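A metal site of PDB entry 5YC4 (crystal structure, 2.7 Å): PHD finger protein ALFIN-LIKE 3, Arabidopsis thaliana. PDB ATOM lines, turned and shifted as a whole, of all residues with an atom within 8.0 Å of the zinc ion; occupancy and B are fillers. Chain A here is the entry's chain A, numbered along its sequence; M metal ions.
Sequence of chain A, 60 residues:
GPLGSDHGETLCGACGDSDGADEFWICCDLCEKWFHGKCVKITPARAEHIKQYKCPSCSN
Four residues have an atom within 4 Å of the zinc ion: Cys 12, Cys 15, His 36 and Cys 39.
The zinc ion is bound by a ring nitrogen (ND1) of His 36 (2.2 Å), the side-chain sulfur of Cys 39 (2.3 Å), the side-chain sulfur of Cys 12 (2.4 Å) and the side-chain sulfur of Cys 15 (2.4 Å). The zinc ion has four donor atoms within binding distance.
A ring nitrogen (NE2) of His 36 sits at hydrogen-bond distance from the side-chain carboxylate (OE1) of Glu 23 (3.1 Å). N of Ala 14 lies close to SG of Cys 12 (3.4 Å). O of Asp 17 is in hydrogen-bond range of N of Cys 12 (2.9 Å). The backbone NH of Asp 17 sits close to the side-chain sulfur of Cys 15 (3.5 Å).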
ATOM      1  N   LEU A  11     -19.187  17.320  21.112  1.00  0.00           N
ATOM      2  CA  LEU A  11     -20.630  17.324  20.961  1.00  0.00           C
ATOM      3  C   LEU A  11     -21.337  17.231  22.309  1.00  0.00           C
ATOM      4  O   LEU A  11     -20.979  16.412  23.158  1.00  0.00           O
ATOM      5  CB  LEU A  11     -21.076  16.175  20.062  1.00  0.00           C
ATOM      6  CG  LEU A  11     -20.520  16.181  18.634  1.00  0.00           C
ATOM      7  CD1 LEU A  11     -21.011  14.976  17.861  1.00  0.00           C
ATOM      8  CD2 LEU A  11     -20.889  17.473  17.911  1.00  0.00           C
ATOM      9  N   CYS A  12     -22.337  18.093  22.501  1.00  0.00           N
ATOM     10  CA  CYS A  12     -23.140  18.069  23.716  1.00  0.00           C
ATOM     11  C   CYS A  12     -23.884  16.736  23.818  1.00  0.00           C
ATOM     12  O   CYS A  12     -24.441  16.252  22.836  1.00  0.00           O
ATOM     13  CB  CYS A  12     -24.137  19.234  23.726  1.00  0.00           C
ATOM     14  SG  CYS A  12     -25.239  19.257  25.166  1.00  0.00           S
ATOM     15  N   GLY A  13     -23.898  16.157  25.018  1.00  0.00           N
ATOM     16  CA  GLY A  13     -24.509  14.858  25.218  1.00  0.00           C
ATOM     17  C   GLY A  13     -26.027  14.889  25.238  1.00  0.00           C
ATOM     18  O   GLY A  13     -26.675  13.851  25.322  1.00  0.00           O
ATOM     19  N   ALA A  14     -26.601  16.093  25.147  1.00  0.00           N
ATOM     20  CA  ALA A  14     -28.046  16.255  25.189  1.00  0.00           C
ATOM     21  C   ALA A  14     -28.623  16.640  23.825  1.00  0.00           C
ATOM     22  O   ALA A  14     -29.518  15.980  23.316  1.00  0.00           O
ATOM     23  CB  ALA A  14     -28.435  17.288  26.244  1.00  0.00           C
ATOM     24  N   CYS A  15     -28.102  17.723  23.247  1.00  0.00           N
ATOM     25  CA  CYS A  15     -28.632  18.225  21.990  1.00  0.00           C
ATOM     26  C   CYS A  15     -27.814  17.760  20.784  1.00  0.00           C
ATOM     27  O   CYS A  15     -28.278  17.827  19.645  1.00  0.00           O
ATOM     28  CB  CYS A  15     -28.687  19.756  22.010  1.00  0.00           C
ATOM     29  SG  CYS A  15     -27.084  20.570  22.099  1.00  0.00           S
ATOM     30  N   GLY A  16     -26.607  17.285  21.043  1.00  0.00           N
ATOM     31  CA  GLY A  16     -25.752  16.768  19.988  1.00  0.00           C
ATOM     32  C   GLY A  16     -25.114  17.846  19.128  1.00  0.00           C
ATOM     33  O   GLY A  16     -24.583  17.557  18.056  1.00  0.00           O
ATOM     34  N   ASP A  17     -25.170  19.090  19.587  1.00  0.00           N
ATOM     35  CA  ASP A  17     -24.590  20.205  18.842  1.00  0.00           C
ATOM     36  C   ASP A  17     -23.129  20.454  19.240  1.00  0.00           C
ATOM     37  O   ASP A  17     -22.665  19.952  20.267  1.00  0.00           O
ATOM     38  CB  ASP A  17     -25.401  21.480  19.062  1.00  0.00           C
ATOM     39  CG  ASP A  17     -26.600  21.572  18.141  1.00  0.00           C
ATOM     40  OD1 ASP A  17     -27.011  20.528  17.587  1.00  0.00           O
ATOM     41  OD2 ASP A  17     -27.151  22.679  17.978  1.00  0.00           O
ATOM     42  N   SER A  18     -22.427  21.220  18.422  1.00  0.00           N
ATOM     43  CA  SER A  18     -21.027  21.544  18.677  1.00  0.00           C
ATOM     44  C   SER A  18     -20.914  22.740  19.612  1.00  0.00           C
ATOM     45  O   SER A  18     -21.903  23.429  19.885  1.00  0.00           O
ATOM     46  CB  SER A  18     -20.290  21.825  17.368  1.00  0.00           C
ATOM     47  OG  SER A  18     -20.529  20.792  16.423  1.00  0.00           O
ATOM     48  N   GLU A  23     -20.235  30.089  25.700  1.00  0.00           N
ATOM     49  CA  GLU A  23     -21.138  29.076  26.229  1.00  0.00           C
ATOM     50  C   GLU A  23     -20.543  28.397  27.456  1.00  0.00           C
ATOM     51  O   GLU A  23     -19.347  28.110  27.489  1.00  0.00           O
ATOM     52  CB  GLU A  23     -21.466  28.029  25.171  1.00  0.00           C
ATOM     53  CG  GLU A  23     -22.166  28.585  23.935  1.00  0.00           C
ATOM     54  CD  GLU A  23     -22.359  27.521  22.872  1.00  0.00           C
ATOM     55  OE1 GLU A  23     -21.791  26.423  23.010  1.00  0.00           O
ATOM     56  OE2 GLU A  23     -23.076  27.798  21.892  1.00  0.00           O
ATOM     57  N   PHE A  24     -21.381  28.135  28.453  1.00  0.00           N
ATOM     58  CA  PHE A  24     -20.931  27.424  29.643  1.00  0.00           C
ATOM     59  C   PHE A  24     -21.135  25.924  29.476  1.00  0.00           C
ATOM     60  O   PHE A  24     -22.231  25.464  29.151  1.00  0.00           O
ATOM     61  CB  PHE A  24     -21.664  27.925  30.889  1.00  0.00           C
ATOM     62  CG  PHE A  24     -21.287  27.191  32.148  1.00  0.00           C
ATOM     63  CD1 PHE A  24     -20.071  27.443  32.770  1.00  0.00           C
ATOM     64  CD2 PHE A  24     -22.132  26.259  32.708  1.00  0.00           C
ATOM     65  CE1 PHE A  24     -19.716  26.768  33.927  1.00  0.00           C
ATOM     66  CE2 PHE A  24     -21.790  25.589  33.861  1.00  0.00           C
ATOM     67  CZ  PHE A  24     -20.580  25.839  34.471  1.00  0.00           C
ATOM     68  N   TRP A  25     -20.080  25.162  29.707  1.00  0.00           N
ATOM     69  CA  TRP A  25     -20.126  23.710  29.553  1.00  0.00           C
ATOM     70  C   TRP A  25     -19.750  23.018  30.861  1.00  0.00           C
ATOM     71  O   TRP A  25     -19.052  23.591  31.698  1.00  0.00           O
ATOM     72  CB  TRP A  25     -19.184  23.255  28.439  1.00  0.00           C
ATOM     73  CG  TRP A  25     -19.698  23.537  27.055  1.00  0.00           C
ATOM     74  CD1 TRP A  25     -19.803  24.757  26.452  1.00  0.00           C
ATOM     75  CD2 TRP A  25     -20.145  22.576  26.092  1.00  0.00           C
ATOM     76  NE1 TRP A  25     -20.301  24.615  25.184  1.00  0.00           N
ATOM     77  CE2 TRP A  25     -20.516  23.287  24.937  1.00  0.00           C
ATOM     78  CE3 TRP A  25     -20.266  21.183  26.105  1.00  0.00           C
ATOM     79  CZ2 TRP A  25     -21.004  22.642  23.801  1.00  0.00           C
ATOM     80  CZ3 TRP A  25     -20.749  20.551  24.973  1.00  0.00           C
ATOM     81  CH2 TRP A  25     -21.117  21.286  23.844  1.00  0.00           C
ATOM     82  N   TRP A  34     -19.599  15.794  27.572  1.00  0.00           N
ATOM     83  CA  TRP A  34     -19.780  17.218  27.812  1.00  0.00           C
ATOM     84  C   TRP A  34     -21.217  17.635  27.528  1.00  0.00           C
ATOM     85  O   TRP A  34     -21.899  17.058  26.684  1.00  0.00           O
ATOM     86  CB  TRP A  34     -18.826  18.033  26.939  1.00  0.00           C
ATOM     87  CG  TRP A  34     -17.431  18.127  27.483  1.00  0.00           C
ATOM     88  CD1 TRP A  34     -16.373  17.329  27.149  1.00  0.00           C
ATOM     89  CD2 TRP A  34     -16.939  19.065  28.445  1.00  0.00           C
ATOM     90  NE1 TRP A  34     -15.254  17.711  27.848  1.00  0.00           N
ATOM     91  CE2 TRP A  34     -15.575  18.771  28.653  1.00  0.00           C
ATOM     92  CE3 TRP A  34     -17.522  20.120  29.151  1.00  0.00           C
ATOM     93  CZ2 TRP A  34     -14.781  19.507  29.535  1.00  0.00           C
ATOM     94  CZ3 TRP A  34     -16.723  20.847  30.032  1.00  0.00           C
ATOM     95  CH2 TRP A  34     -15.375  20.536  30.212  1.00  0.00           C
ATOM     96  N   PHE A  35     -21.668  18.661  28.258  1.00  0.00           N
ATOM     97  CA  PHE A  35     -23.028  19.152  28.114  1.00  0.00           C
ATOM     98  C   PHE A  35     -23.070  20.677  28.170  1.00  0.00           C
ATOM     99  O   PHE A  35     -22.296  21.288  28.909  1.00  0.00           O
ATOM    100  CB  PHE A  35     -23.933  18.582  29.221  1.00  0.00           C
ATOM    101  CG  PHE A  35     -23.932  17.079  29.284  1.00  0.00           C
ATOM    102  CD1 PHE A  35     -22.996  16.402  30.053  1.00  0.00           C
ATOM    103  CD2 PHE A  35     -24.889  16.342  28.596  1.00  0.00           C
ATOM    104  CE1 PHE A  35     -23.000  15.017  30.112  1.00  0.00           C
ATOM    105  CE2 PHE A  35     -24.895  14.956  28.665  1.00  0.00           C
ATOM    106  CZ  PHE A  35     -23.949  14.294  29.419  1.00  0.00           C
ATOM    107  N   HIS A  36     -23.958  21.278  27.392  1.00  0.00           N
ATOM    108  CA  HIS A  36     -24.280  22.685  27.567  1.00  0.00           C
ATOM    109  C   HIS A  36     -24.853  22.881  28.959  1.00  0.00           C
ATOM    110  O   HIS A  36     -25.632  22.057  29.429  1.00  0.00           O
ATOM    111  CB  HIS A  36     -25.298  23.169  26.532  1.00  0.00           C
ATOM    112  CG  HIS A  36     -24.744  23.349  25.152  1.00  0.00           C
ATOM    113  ND1 HIS A  36     -24.950  22.431  24.140  1.00  0.00           N
ATOM    114  CD2 HIS A  36     -24.000  24.345  24.605  1.00  0.00           C
ATOM    115  CE1 HIS A  36     -24.361  22.848  23.042  1.00  0.00           C
ATOM    116  NE2 HIS A  36     -23.771  24.004  23.288  1.00  0.00           N
ATOM    117  N   GLY A  37     -24.482  23.981  29.617  1.00  0.00           N
ATOM    118  CA  GLY A  37     -25.066  24.318  30.902  1.00  0.00           C
ATOM    119  C   GLY A  37     -26.561  24.562  30.764  1.00  0.00           C
ATOM    120  O   GLY A  37     -27.340  24.230  31.651  1.00  0.00           O
ATOM    121  N   LYS A  38     -26.942  25.126  29.623  1.00  0.00           N
ATOM    122  CA  LYS A  38     -28.343  25.416  29.330  1.00  0.00           C
ATOM    123  C   LYS A  38     -29.166  24.144  29.134  1.00  0.00           C
ATOM    124  O   LYS A  38     -30.351  24.096  29.472  1.00  0.00           O
ATOM    125  CB  LYS A  38     -28.456  26.280  28.075  1.00  0.00           C
ATOM    126  CG  LYS A  38     -27.865  27.681  28.213  1.00  0.00           C
ATOM    127  CD  LYS A  38     -28.679  28.526  29.175  1.00  0.00           C
ATOM    128  CE  LYS A  38     -28.199  29.968  29.192  1.00  0.00           C
ATOM    129  NZ  LYS A  38     -28.304  30.597  27.849  1.00  0.00           N
ATOM    130  N   CYS A  39     -28.537  23.115  28.583  1.00  0.00           N
ATOM    131  CA  CYS A  39     -29.235  21.869  28.269  1.00  0.00           C
ATOM    132  C   CYS A  39     -29.527  21.044  29.516  1.00  0.00           C
ATOM    133  O   CYS A  39     -30.595  20.441  29.630  1.00  0.00           O
ATOM    134  CB  CYS A  39     -28.426  21.044  27.267  1.00  0.00           C
ATOM    135  SG  CYS A  39     -28.427  21.751  25.608  1.00  0.00           S
ATOM    136  N   VAL A  40     -28.585  21.022  30.457  1.00  0.00           N
ATOM    137  CA  VAL A  40     -28.797  20.320  31.715  1.00  0.00           C
ATOM    138  C   VAL A  40     -29.278  21.278  32.794  1.00  0.00           C
ATOM    139  O   VAL A  40     -29.323  20.938  33.982  1.00  0.00           O
ATOM    140  CB  VAL A  40     -27.504  19.613  32.205  1.00  0.00           C
ATOM    141  CG1 VAL A  40     -27.162  18.445  31.283  1.00  0.00           C
ATOM    142  CG2 VAL A  40     -26.352  20.598  32.283  1.00  0.00           C
HETATM  143 ZN    ZN M   1     -26.607  21.078  24.402  1.00  0.00          ZN
